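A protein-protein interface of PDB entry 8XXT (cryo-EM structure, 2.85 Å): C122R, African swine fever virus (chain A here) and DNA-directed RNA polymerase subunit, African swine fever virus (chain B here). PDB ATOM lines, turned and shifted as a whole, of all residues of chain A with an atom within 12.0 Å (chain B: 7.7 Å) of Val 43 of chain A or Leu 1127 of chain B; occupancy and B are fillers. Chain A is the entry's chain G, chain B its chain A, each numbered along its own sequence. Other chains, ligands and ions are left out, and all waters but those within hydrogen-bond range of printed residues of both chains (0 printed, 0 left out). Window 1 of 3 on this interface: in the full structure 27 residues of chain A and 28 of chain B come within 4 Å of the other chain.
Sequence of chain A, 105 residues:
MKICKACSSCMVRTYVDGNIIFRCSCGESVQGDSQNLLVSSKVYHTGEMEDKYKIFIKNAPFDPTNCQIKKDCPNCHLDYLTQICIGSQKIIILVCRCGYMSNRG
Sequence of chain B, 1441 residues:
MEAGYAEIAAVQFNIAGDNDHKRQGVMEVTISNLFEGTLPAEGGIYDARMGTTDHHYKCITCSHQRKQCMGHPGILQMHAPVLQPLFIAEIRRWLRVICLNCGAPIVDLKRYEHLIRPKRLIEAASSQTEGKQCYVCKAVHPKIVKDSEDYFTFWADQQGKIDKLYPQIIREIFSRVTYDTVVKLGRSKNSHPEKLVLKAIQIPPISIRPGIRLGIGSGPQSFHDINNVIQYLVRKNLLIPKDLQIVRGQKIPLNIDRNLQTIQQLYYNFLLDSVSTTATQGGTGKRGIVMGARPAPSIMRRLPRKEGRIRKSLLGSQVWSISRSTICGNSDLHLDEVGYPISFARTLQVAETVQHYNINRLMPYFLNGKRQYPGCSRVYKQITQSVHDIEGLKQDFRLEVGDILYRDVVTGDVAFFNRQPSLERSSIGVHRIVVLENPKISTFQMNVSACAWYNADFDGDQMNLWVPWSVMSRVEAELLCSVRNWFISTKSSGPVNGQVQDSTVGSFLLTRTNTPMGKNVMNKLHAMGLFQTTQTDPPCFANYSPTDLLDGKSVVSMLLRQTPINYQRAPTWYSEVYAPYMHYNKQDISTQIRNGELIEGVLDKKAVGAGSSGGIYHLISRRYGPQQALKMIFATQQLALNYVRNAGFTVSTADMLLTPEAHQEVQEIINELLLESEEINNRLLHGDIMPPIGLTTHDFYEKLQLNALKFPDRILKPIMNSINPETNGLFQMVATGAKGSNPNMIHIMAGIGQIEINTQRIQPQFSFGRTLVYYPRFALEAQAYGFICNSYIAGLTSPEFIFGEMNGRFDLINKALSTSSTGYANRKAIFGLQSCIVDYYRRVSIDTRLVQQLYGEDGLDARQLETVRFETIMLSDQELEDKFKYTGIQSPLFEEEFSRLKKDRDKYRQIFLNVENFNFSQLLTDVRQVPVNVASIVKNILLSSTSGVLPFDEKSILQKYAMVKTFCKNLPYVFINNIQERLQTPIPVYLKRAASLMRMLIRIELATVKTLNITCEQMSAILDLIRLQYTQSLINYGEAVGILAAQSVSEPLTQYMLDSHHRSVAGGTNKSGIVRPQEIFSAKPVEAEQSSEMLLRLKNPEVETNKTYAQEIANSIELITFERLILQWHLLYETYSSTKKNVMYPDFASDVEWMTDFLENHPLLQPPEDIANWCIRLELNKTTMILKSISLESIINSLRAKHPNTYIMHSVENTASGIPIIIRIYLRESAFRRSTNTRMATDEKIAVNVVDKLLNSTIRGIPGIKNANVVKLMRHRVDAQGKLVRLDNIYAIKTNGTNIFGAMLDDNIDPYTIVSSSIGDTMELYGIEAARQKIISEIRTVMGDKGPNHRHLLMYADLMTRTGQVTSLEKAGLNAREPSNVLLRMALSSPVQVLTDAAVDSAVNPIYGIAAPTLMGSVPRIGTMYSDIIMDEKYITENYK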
ATOM      1  N   LEU A  38       5.363 -17.477  -8.279  1.00  0.00           N
ATOM      2  CA  LEU A  38       6.257 -16.517  -8.921  1.00  0.00           C
ATOM      3  C   LEU A  38       6.008 -16.542 -10.422  1.00  0.00           C
ATOM      4  O   LEU A  38       6.483 -17.434 -11.128  1.00  0.00           O
ATOM      5  CB  LEU A  38       7.710 -16.843  -8.601  1.00  0.00           C
ATOM      6  CG  LEU A  38       8.739 -15.764  -8.938  1.00  0.00           C
ATOM      7  CD1 LEU A  38       8.392 -14.461  -8.245  1.00  0.00           C
ATOM      8  CD2 LEU A  38      10.134 -16.224  -8.553  1.00  0.00           C
ATOM      9  N   VAL A  39       5.263 -15.558 -10.919  1.00  0.00           N
ATOM     10  CA  VAL A  39       4.944 -15.517 -12.341  1.00  0.00           C
ATOM     11  C   VAL A  39       6.144 -15.039 -13.146  1.00  0.00           C
ATOM     12  O   VAL A  39       6.564 -15.690 -14.109  1.00  0.00           O
ATOM     13  CB  VAL A  39       3.709 -14.632 -12.583  1.00  0.00           C
ATOM     14  CG1 VAL A  39       3.746 -14.017 -13.974  1.00  0.00           C
ATOM     15  CG2 VAL A  39       2.442 -15.433 -12.387  1.00  0.00           C
ATOM     16  N   SER A  40       6.718 -13.902 -12.763  1.00  0.00           N
ATOM     17  CA  SER A  40       7.863 -13.349 -13.471  1.00  0.00           C
ATOM     18  C   SER A  40       8.638 -12.453 -12.521  1.00  0.00           C
ATOM     19  O   SER A  40       8.100 -11.953 -11.530  1.00  0.00           O
ATOM     20  CB  SER A  40       7.430 -12.572 -14.718  1.00  0.00           C
ATOM     21  OG  SER A  40       8.389 -12.697 -15.754  1.00  0.00           O
ATOM     22  N   SER A  41       9.915 -12.251 -12.840  1.00  0.00           N
ATOM     23  CA  SER A  41      10.785 -11.448 -11.996  1.00  0.00           C
ATOM     24  C   SER A  41      11.881 -10.826 -12.846  1.00  0.00           C
ATOM     25  O   SER A  41      12.190 -11.297 -13.944  1.00  0.00           O
ATOM     26  CB  SER A  41      11.402 -12.282 -10.871  1.00  0.00           C
ATOM     27  OG  SER A  41      12.335 -13.217 -11.381  1.00  0.00           O
ATOM     28  N   LYS A  42      12.464  -9.753 -12.319  1.00  0.00           N
ATOM     29  CA  LYS A  42      13.597  -9.093 -12.950  1.00  0.00           C
ATOM     30  C   LYS A  42      14.403  -8.390 -11.874  1.00  0.00           C
ATOM     31  O   LYS A  42      13.857  -7.589 -11.111  1.00  0.00           O
ATOM     32  CB  LYS A  42      13.145  -8.094 -14.018  1.00  0.00           C
ATOM     33  CG  LYS A  42      14.278  -7.551 -14.876  1.00  0.00           C
ATOM     34  CD  LYS A  42      14.956  -8.658 -15.668  1.00  0.00           C
ATOM     35  CE  LYS A  42      14.003  -9.298 -16.664  1.00  0.00           C
ATOM     36  NZ  LYS A  42      13.707  -8.396 -17.811  1.00  0.00           N
ATOM     37  N   VAL A  43      15.694  -8.697 -11.812  1.00  0.00           N
ATOM     38  CA  VAL A  43      16.604  -8.098 -10.847  1.00  0.00           C
ATOM     39  C   VAL A  43      17.657  -7.319 -11.620  1.00  0.00           C
ATOM     40  O   VAL A  43      18.288  -7.859 -12.535  1.00  0.00           O
ATOM     41  CB  VAL A  43      17.254  -9.159  -9.941  1.00  0.00           C
ATOM     42  CG1 VAL A  43      18.003  -8.493  -8.807  1.00  0.00           C
ATOM     43  CG2 VAL A  43      16.197 -10.106  -9.398  1.00  0.00           C
ATOM     44  N   TYR A  44      17.839  -6.055 -11.256  1.00  0.00           N
ATOM     45  CA  TYR A  44      18.717  -5.156 -11.990  1.00  0.00           C
ATOM     46  C   TYR A  44      20.133  -5.202 -11.434  1.00  0.00           C
ATOM     47  O   TYR A  44      20.337  -5.286 -10.218  1.00  0.00           O
ATOM     48  CB  TYR A  44      18.170  -3.731 -11.944  1.00  0.00           C
ATOM     49  CG  TYR A  44      16.812  -3.613 -12.585  1.00  0.00           C
ATOM     50  CD1 TYR A  44      16.654  -3.804 -13.949  1.00  0.00           C
ATOM     51  CD2 TYR A  44      15.684  -3.337 -11.828  1.00  0.00           C
ATOM     52  CE1 TYR A  44      15.418  -3.708 -14.544  1.00  0.00           C
ATOM     53  CE2 TYR A  44      14.440  -3.238 -12.416  1.00  0.00           C
ATOM     54  CZ  TYR A  44      14.316  -3.426 -13.774  1.00  0.00           C
ATOM     55  OH  TYR A  44      13.083  -3.330 -14.371  1.00  0.00           O
ATOM     56  N   HIS A  45      21.106  -5.142 -12.343  1.00  0.00           N
ATOM     57  CA  HIS A  45      22.526  -5.248 -12.014  1.00  0.00           C
ATOM     58  C   HIS A  45      22.806  -6.518 -11.216  1.00  0.00           C
ATOM     59  O   HIS A  45      23.511  -6.514 -10.205  1.00  0.00           O
ATOM     60  CB  HIS A  45      23.018  -4.006 -11.270  1.00  0.00           C
ATOM     61  CG  HIS A  45      24.479  -3.737 -11.452  1.00  0.00           C
ATOM     62  ND1 HIS A  45      25.199  -4.237 -12.516  1.00  0.00           N
ATOM     63  CD2 HIS A  45      25.353  -3.013 -10.713  1.00  0.00           C
ATOM     64  CE1 HIS A  45      26.454  -3.839 -12.422  1.00  0.00           C
ATOM     65  NE2 HIS A  45      26.575  -3.095 -11.338  1.00  0.00           N
ATOM     66  N   THR A  46      22.228  -7.621 -11.685  1.00  0.00           N
ATOM     67  CA  THR A  46      22.449  -8.938 -11.112  1.00  0.00           C
ATOM     68  C   THR A  46      22.567  -9.934 -12.257  1.00  0.00           C
ATOM     69  O   THR A  46      22.043  -9.705 -13.350  1.00  0.00           O
ATOM     70  CB  THR A  46      21.321  -9.326 -10.145  1.00  0.00           C
ATOM     71  OG1 THR A  46      21.089  -8.244  -9.235  1.00  0.00           O
ATOM     72  CG2 THR A  46      21.690 -10.565  -9.340  1.00  0.00           C
ATOM     73  N   GLY A  47      23.261 -11.040 -12.000  1.00  0.00           N
ATOM     74  CA  GLY A  47      23.661 -11.930 -13.071  1.00  0.00           C
ATOM     75  C   GLY A  47      24.891 -11.461 -13.803  1.00  0.00           C
ATOM     76  O   GLY A  47      25.143 -11.901 -14.929  1.00  0.00           O
ATOM     77  N   GLU A  48      25.652 -10.555 -13.198  1.00  0.00           N
ATOM     78  CA  GLU A  48      26.867 -10.012 -13.781  1.00  0.00           C
ATOM     79  C   GLU A  48      27.966 -10.039 -12.734  1.00  0.00           C
ATOM     80  O   GLU A  48      27.750  -9.595 -11.603  1.00  0.00           O
ATOM     81  CB  GLU A  48      26.654  -8.575 -14.270  1.00  0.00           C
ATOM     82  CG  GLU A  48      27.900  -7.937 -14.848  1.00  0.00           C
ATOM     83  CD  GLU A  48      27.688  -7.423 -16.252  1.00  0.00           C
ATOM     84  OE1 GLU A  48      28.544  -7.690 -17.120  1.00  0.00           O
ATOM     85  OE2 GLU A  48      26.665  -6.748 -16.487  1.00  0.00           O
ATOM     86  N   MET A  49      29.148 -10.510 -13.135  1.00  0.00           N
ATOM     87  CA  MET A  49      30.402 -10.583 -12.396  1.00  0.00           C
ATOM     88  C   MET A  49      30.386 -11.857 -11.521  1.00  0.00           C
ATOM     89  O   MET A  49      31.327 -12.084 -10.769  1.00  0.00           O
ATOM     90  CB  MET A  49      30.650  -9.339 -11.508  1.00  0.00           C
ATOM     91  CG  MET A  49      31.910  -9.197 -10.606  1.00  0.00           C
ATOM     92  SD  MET A  49      33.547  -9.382 -11.391  1.00  0.00           S
ATOM     93  CE  MET A  49      33.832 -11.120 -11.612  1.00  0.00           C
ATOM     94  N   GLU A  50      29.331 -12.678 -11.564  1.00  0.00           N
ATOM     95  CA  GLU A  50      29.391 -13.988 -10.918  1.00  0.00           C
ATOM     96  C   GLU A  50      29.329 -15.139 -11.917  1.00  0.00           C
ATOM     97  O   GLU A  50      30.181 -16.029 -11.887  1.00  0.00           O
ATOM     98  CB  GLU A  50      28.279 -14.201  -9.868  1.00  0.00           C
ATOM     99  CG  GLU A  50      27.983 -13.098  -8.836  1.00  0.00           C
ATOM    100  CD  GLU A  50      27.709 -11.742  -9.439  1.00  0.00           C
ATOM    101  OE1 GLU A  50      26.866 -11.691 -10.357  1.00  0.00           O
ATOM    102  OE2 GLU A  50      28.342 -10.742  -9.029  1.00  0.00           O
ATOM    103  N   ASP A  51      28.327 -15.147 -12.795  1.00  0.00           N
ATOM    104  CA  ASP A  51      28.104 -16.275 -13.692  1.00  0.00           C
ATOM    105  C   ASP A  51      28.714 -16.085 -15.070  1.00  0.00           C
ATOM    106  O   ASP A  51      28.946 -17.073 -15.773  1.00  0.00           O
ATOM    107  CB  ASP A  51      26.603 -16.532 -13.856  1.00  0.00           C
ATOM    108  CG  ASP A  51      25.842 -15.281 -14.228  1.00  0.00           C
ATOM    109  OD1 ASP A  51      26.426 -14.187 -14.102  1.00  0.00           O
ATOM    110  OD2 ASP A  51      24.666 -15.387 -14.634  1.00  0.00           O
ATOM    111  N   PHE B1122      10.444   5.030 -12.757  1.00  0.00           N
ATOM    112  CA  PHE B1122      10.484   4.005 -11.717  1.00  0.00           C
ATOM    113  C   PHE B1122      11.677   3.072 -11.882  1.00  0.00           C
ATOM    114  O   PHE B1122      12.334   2.718 -10.896  1.00  0.00           O
ATOM    115  CB  PHE B1122       9.198   3.187 -11.725  1.00  0.00           C
ATOM    116  CG  PHE B1122       8.686   2.863 -10.359  1.00  0.00           C
ATOM    117  CD1 PHE B1122       9.562   2.691  -9.306  1.00  0.00           C
ATOM    118  CD2 PHE B1122       7.340   2.661 -10.140  1.00  0.00           C
ATOM    119  CE1 PHE B1122       9.100   2.374  -8.048  1.00  0.00           C
ATOM    120  CE2 PHE B1122       6.878   2.334  -8.889  1.00  0.00           C
ATOM    121  CZ  PHE B1122       7.755   2.195  -7.841  1.00  0.00           C
ATOM    122  N   GLU B1123      11.969   2.663 -13.119  1.00  0.00           N
ATOM    123  CA  GLU B1123      12.916   1.577 -13.355  1.00  0.00           C
ATOM    124  C   GLU B1123      14.273   1.847 -12.721  1.00  0.00           C
ATOM    125  O   GLU B1123      14.924   0.916 -12.236  1.00  0.00           O
ATOM    126  CB  GLU B1123      13.081   1.346 -14.857  1.00  0.00           C
ATOM    127  CG  GLU B1123      12.092   0.365 -15.456  1.00  0.00           C
ATOM    128  CD  GLU B1123      11.751   0.698 -16.897  1.00  0.00           C
ATOM    129  OE1 GLU B1123      11.055  -0.110 -17.548  1.00  0.00           O
ATOM    130  OE2 GLU B1123      12.181   1.768 -17.376  1.00  0.00           O
ATOM    131  N   ARG B1124      14.716   3.103 -12.708  1.00  0.00           N
ATOM    132  CA  ARG B1124      16.014   3.421 -12.132  1.00  0.00           C
ATOM    133  C   ARG B1124      15.979   3.526 -10.613  1.00  0.00           C
ATOM    134  O   ARG B1124      17.042   3.568  -9.986  1.00  0.00           O
ATOM    135  CB  ARG B1124      16.553   4.717 -12.739  1.00  0.00           C
ATOM    136  CG  ARG B1124      15.935   5.979 -12.184  1.00  0.00           C
ATOM    137  CD  ARG B1124      15.769   7.013 -13.288  1.00  0.00           C
ATOM    138  NE  ARG B1124      17.038   7.567 -13.744  1.00  0.00           N
ATOM    139  CZ  ARG B1124      17.809   8.373 -13.026  1.00  0.00           C
ATOM    140  NH1 ARG B1124      17.465   8.755 -11.807  1.00  0.00           N
ATOM    141  NH2 ARG B1124      18.953   8.807 -13.544  1.00  0.00           N
ATOM    142  N   LEU B1125      14.791   3.559 -10.008  1.00  0.00           N
ATOM    143  CA  LEU B1125      14.676   3.547  -8.556  1.00  0.00           C
ATOM    144  C   LEU B1125      14.532   2.143  -7.984  1.00  0.00           C
ATOM    145  O   LEU B1125      14.433   1.999  -6.762  1.00  0.00           O
ATOM    146  CB  LEU B1125      13.481   4.394  -8.111  1.00  0.00           C
ATOM    147  CG  LEU B1125      13.403   5.831  -8.621  1.00  0.00           C
ATOM    148  CD1 LEU B1125      12.116   6.470  -8.162  1.00  0.00           C
ATOM    149  CD2 LEU B1125      14.589   6.634  -8.135  1.00  0.00           C
ATOM    150  N   ILE B1126      14.522   1.118  -8.830  1.00  0.00           N
ATOM    151  CA  ILE B1126      14.265  -0.256  -8.418  1.00  0.00           C
ATOM    152  C   ILE B1126      15.472  -1.112  -8.764  1.00  0.00           C
ATOM    153  O   ILE B1126      16.077  -0.968  -9.832  1.00  0.00           O
ATOM    154  CB  ILE B1126      12.993  -0.812  -9.092  1.00  0.00           C
ATOM    155  CG1 ILE B1126      11.768  -0.010  -8.666  1.00  0.00           C
ATOM    156  CG2 ILE B1126      12.805  -2.283  -8.776  1.00  0.00           C
ATOM    157  CD1 ILE B1126      10.479  -0.642  -9.097  1.00  0.00           C
ATOM    158  N   LEU B1127      15.827  -2.009  -7.846  1.00  0.00           N
ATOM    159  CA  LEU B1127      16.882  -2.976  -8.097  1.00  0.00           C
ATOM    160  C   LEU B1127      16.369  -4.402  -8.242  1.00  0.00           C
ATOM    161  O   LEU B1127      17.134  -5.269  -8.679  1.00  0.00           O
ATOM    162  CB  LEU B1127      17.952  -2.920  -6.992  1.00  0.00           C
ATOM    163  CG  LEU B1127      17.715  -3.540  -5.615  1.00  0.00           C
ATOM    164  CD1 LEU B1127      18.925  -3.302  -4.733  1.00  0.00           C
ATOM    165  CD2 LEU B1127      16.483  -2.969  -4.951  1.00  0.00           C
ATOM    166  N   GLN B1128      15.109  -4.671  -7.902  1.00  0.00           N
ATOM    167  CA  GLN B1128      14.489  -5.962  -8.169  1.00  0.00           C
ATOM    168  C   GLN B1128      12.988  -5.848  -7.961  1.00  0.00           C
ATOM    169  O   GLN B1128      12.538  -5.194  -7.018  1.00  0.00           O
ATOM    170  CB  GLN B1128      15.058  -7.068  -7.270  1.00  0.00           C
ATOM    171  CG  GLN B1128      15.096  -6.730  -5.794  1.00  0.00           C
ATOM    172  CD  GLN B1128      15.559  -7.898  -4.945  1.00  0.00           C
ATOM    173  OE1 GLN B1128      15.070  -9.017  -5.087  1.00  0.00           O
ATOM    174  NE2 GLN B1128      16.512  -7.642  -4.057  1.00  0.00           N
ATOM    175  N   TRP B1129      12.225  -6.484  -8.846  1.00  0.00           N
ATOM    176  CA  TRP B1129      10.779  -6.565  -8.710  1.00  0.00           C
ATOM    177  C   TRP B1129      10.325  -7.982  -9.016  1.00  0.00           C
ATOM    178  O   TRP B1129      10.981  -8.714  -9.762  1.00  0.00           O
ATOM    179  CB  TRP B1129      10.053  -5.568  -9.625  1.00  0.00           C
ATOM    180  CG  TRP B1129      10.275  -5.777 -11.093  1.00  0.00           C
ATOM    181  CD1 TRP B1129      11.141  -5.096 -11.888  1.00  0.00           C
ATOM    182  CD2 TRP B1129       9.605  -6.717 -11.945  1.00  0.00           C
ATOM    183  NE1 TRP B1129      11.064  -5.555 -13.177  1.00  0.00           N
ATOM    184  CE2 TRP B1129      10.127  -6.551 -13.238  1.00  0.00           C
ATOM    185  CE3 TRP B1129       8.620  -7.685 -11.736  1.00  0.00           C
ATOM    186  CZ2 TRP B1129       9.698  -7.316 -14.319  1.00  0.00           C
ATOM    187  CZ3 TRP B1129       8.199  -8.444 -12.808  1.00  0.00           C
ATOM    188  CH2 TRP B1129       8.736  -8.255 -14.084  1.00  0.00           C
ATOM    189  N   HIS B1130       9.188  -8.363  -8.436  1.00  0.00           N
ATOM    190  CA  HIS B1130       8.645  -9.702  -8.598  1.00  0.00           C
ATOM    191  C   HIS B1130       7.144  -9.632  -8.826  1.00  0.00           C
ATOM    192  O   HIS B1130       6.439  -8.888  -8.141  1.00  0.00           O
ATOM    193  CB  HIS B1130       8.947 -10.570  -7.373  1.00  0.00           C
ATOM    194  CG  HIS B1130      10.404 -10.821  -7.165  1.00  0.00           C
ATOM    195  ND1 HIS B1130      11.050 -11.919  -7.689  1.00  0.00           N
ATOM    196  CD2 HIS B1130      11.346 -10.109  -6.504  1.00  0.00           C
ATOM    197  CE1 HIS B1130      12.327 -11.876  -7.355  1.00  0.00           C
ATOM    198  NE2 HIS B1130      12.532 -10.788  -6.634  1.00  0.00           N
ATOM    199  N   LEU B1178       8.101  -4.743  -5.247  1.00  0.00           N
ATOM    200  CA  LEU B1178       9.278  -4.051  -5.744  1.00  0.00           C
ATOM    201  C   LEU B1178      10.135  -3.575  -4.585  1.00  0.00           C
ATOM    202  O   LEU B1178       9.619  -3.106  -3.568  1.00  0.00           O
ATOM    203  CB  LEU B1178       8.895  -2.863  -6.631  1.00  0.00           C
ATOM    204  CG  LEU B1178       7.532  -2.942  -7.319  1.00  0.00           C
ATOM    205  CD1 LEU B1178       6.597  -1.866  -6.799  1.00  0.00           C
ATOM    206  CD2 LEU B1178       7.681  -2.849  -8.827  1.00  0.00           C
ATOM    207  N   GLU B1179      11.444  -3.709  -4.745  1.00  0.00           N
ATOM    208  CA  GLU B1179      12.417  -3.161  -3.817  1.00  0.00           C
ATOM    209  C   GLU B1179      13.013  -1.895  -4.412  1.00  0.00           C
ATOM    210  O   GLU B1179      13.059  -1.728  -5.633  1.00  0.00           O
ATOM    211  CB  GLU B1179      13.529  -4.168  -3.521  1.00  0.00           C
ATOM    212  CG  GLU B1179      13.179  -5.201  -2.479  1.00  0.00           C
ATOM    213  CD  GLU B1179      14.212  -6.302  -2.387  1.00  0.00           C
ATOM    214  OE1 GLU B1179      15.411  -6.008  -2.570  1.00  0.00           O
ATOM    215  OE2 GLU B1179      13.824  -7.464  -2.143  1.00  0.00           O
ATOM    216  N   LEU B1180      13.468  -1.001  -3.543  1.00  0.00           N
ATOM    217  CA  LEU B1180      14.014   0.281  -3.965  1.00  0.00           C
ATOM    218  C   LEU B1180      15.520   0.317  -3.757  1.00  0.00           C
ATOM    219  O   LEU B1180      16.038  -0.220  -2.774  1.00  0.00           O
ATOM    220  CB  LEU B1180      13.358   1.440  -3.211  1.00  0.00           C
ATOM    221  CG  LEU B1180      11.986   1.953  -3.663  1.00  0.00           C
ATOM    222  CD1 LEU B1180      11.079   0.842  -4.142  1.00  0.00           C
ATOM    223  CD2 LEU B1180      11.315   2.740  -2.549  1.00  0.00           C
ATOM    224  N   ASN B1181      16.219   0.946  -4.696  1.00  0.00           N
ATOM    225  CA  ASN B1181      17.647   1.205  -4.552  1.00  0.00           C
ATOM    226  C   ASN B1181      17.759   2.487  -3.740  1.00  0.00           C
ATOM    227  O   ASN B1181      17.641   3.589  -4.279  1.00  0.00           O
ATOM    228  CB  ASN B1181      18.311   1.313  -5.924  1.00  0.00           C
ATOM    229  CG  ASN B1181      19.756   1.815  -5.870  1.00  0.00           C
ATOM    230  OD1 ASN B1181      20.133   2.642  -5.041  1.00  0.00           O
ATOM    231  ND2 ASN B1181      20.574   1.298  -6.776  1.00  0.00           N
ATOM    232  N   LYS B1182      17.976   2.344  -2.430  1.00  0.00           N
ATOM    233  CA  LYS B1182      18.022   3.512  -1.555  1.00  0.00           C
ATOM    234  C   LYS B1182      19.125   4.476  -1.963  1.00  0.00           C
ATOM    235  O   LYS B1182      18.949   5.694  -1.862  1.00  0.00           O
ATOM    236  CB  LYS B1182      18.211   3.079  -0.102  1.00  0.00           C
ATOM    237  CG  LYS B1182      17.041   2.299   0.478  1.00  0.00           C
ATOM    238  CD  LYS B1182      17.446   1.459   1.688  1.00  0.00           C
ATOM    239  CE  LYS B1182      18.819   1.842   2.225  1.00  0.00           C
ATOM    240  NZ  LYS B1182      19.133   1.154   3.507  1.00  0.00           N
ATOM    241  N   THR B1183      20.259   3.954  -2.436  1.00  0.00           N
ATOM    242  CA  THR B1183      21.356   4.824  -2.845  1.00  0.00           C
ATOM    243  C   THR B1183      20.929   5.753  -3.971  1.00  0.00           C
ATOM    244  O   THR B1183      21.271   6.942  -3.969  1.00  0.00           O
ATOM    245  CB  THR B1183      22.559   3.987  -3.274  1.00  0.00           C
ATOM    246  OG1 THR B1183      22.333   3.468  -4.590  1.00  0.00           O
ATOM    247  CG2 THR B1183      22.774   2.834  -2.306  1.00  0.00           C
ATOM    248  N   PRO B1220      15.660  -3.263   3.128  1.00  0.00           N
ATOM    249  CA  PRO B1220      15.027  -2.839   1.876  1.00  0.00           C
ATOM    250  C   PRO B1220      13.695  -2.153   2.125  1.00  0.00           C
ATOM    251  O   PRO B1220      12.970  -2.481   3.067  1.00  0.00           O
ATOM    252  CB  PRO B1220      14.841  -4.154   1.106  1.00  0.00           C
ATOM    253  CG  PRO B1220      15.729  -5.147   1.793  1.00  0.00           C
ATOM    254  CD  PRO B1220      15.772  -4.727   3.223  1.00  0.00           C
ATOM    255  N   ILE B1221      13.378  -1.191   1.265  1.00  0.00           N
ATOM    256  CA  ILE B1221      12.049  -0.594   1.243  1.00  0.00           C
ATOM    257  C   ILE B1221      11.199  -1.364   0.246  1.00  0.00           C
ATOM    258  O   ILE B1221      11.593  -1.546  -0.911  1.00  0.00           O
ATOM    259  CB  ILE B1221      12.121   0.896   0.881  1.00  0.00           C
ATOM    260  CG1 ILE B1221      13.059   1.629   1.838  1.00  0.00           C
ATOM    261  CG2 ILE B1221      10.738   1.508   0.924  1.00  0.00           C
ATOM    262  CD1 ILE B1221      13.387   3.035   1.407  1.00  0.00           C
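OG1 of Thr 46 of chain A sits at hydrogen-bond distance from O of Tyr 44 of chain A, 3.2 Å away.
The side-chain carboxylate (OE1) of Glu 1179 of chain B sits at hydrogen-bond distance from the side-chain amide nitrogen (NE2) of Gln 1128 of chain B (2.5 Å).
The side-chain amide oxygen of Gln 1128 of chain B sits at hydrogen-bond distance from a ring nitrogen (NE2) of His 1130 of chain B, at 3.5 Å.
Among the printed residues, merely in contact across the chains: Leu 38 of chain A with His 1130 of chain B (3.7 Å), Ser 40 of chain A with Trp 1129 of chain B (3.7 Å), Ser 40 of chain A with His 1130 of chain B (3.7 Å), Ser 41 of chain A with Trp 1129 of chain B (3.5 Å), Ser 41 of chain A with His 1130 of chain B (3.2 Å), Lys 42 of chain A with Gln 1128 of chain B (3.4 Å), Val 43 of chain A with Leu 1127 of chain B (3.3 Å), Val 43 of chain A with Gln 1128 of chain B (3.6 Å), Tyr 44 of chain A with Glu 1123 of chain B (3.98 Å) and Tyr 44 of chain A with Ile 1126 of chain B (3.1 Å).
Of the 17 printed residues of chain B, 6 touch a printed residue of chain A.
Printed residues of chain B that touch a printed residue of chain A: Glu 1123, Ile 1126, Leu 1127, Gln 1128, Trp 1129 and His 1130.
Hydrophobic or aromatic side chains of chain B within 4 Å of the printed part of chain A: Trp 1129 and His 1130.
Of the 14 printed residues of chain A, 6 touch a printed residue of chain B.
Among the printed residues, no Asp or Glu carboxylate lies within 4 Å of a Lys or Arg side-chain nitrogen of the other chain.
Printed residues of chain B within 4 Å of Ser 41 of chain A: Trp 1129 and His 1130.
Of the printed residues of chain B, Lys 42 of chain A touches Gln 1128 and Trp 1129.
Val 43 of chain A touches just these residues of chain B: Leu 1127 and Gln 1128.
Of the printed residues of chain B, Tyr 44 of chain A touches Glu 1123, Ile 1126, Leu 1127 and Trp 1129.
Thr 46 of chain A touches none of the printed residues of chain B.
Of the printed residues of chain A, Ile 1126 of chain B touches Tyr 44.
Leu 1127 of chain B touches just these residues of chain A: Val 43 and Tyr 44.
No residue of chain A comes within 4 Å of Glu 1179 of chain B.
Asn 1181 of chain B touches none of the printed residues of chain A.
The nearest residue of chain A that does not touch Leu 1127 of chain B is Lys 42 of chain A (4.7 Å).
The backbone carbonyl oxygen of Lys 42 of chain A lies within hydrogen-bond range of the backbone NH of Trp 1129 of chain B, 3.0 Å away.
The backbone carbonyl oxygen of Leu 1127 of chain B sits at hydrogen-bond distance from the backbone NH of Tyr 44 of chain A, 2.8 Å away.
NE1 of Trp 1129 of chain B lies within hydrogen-bond range of OH of Tyr 44 of chain A.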
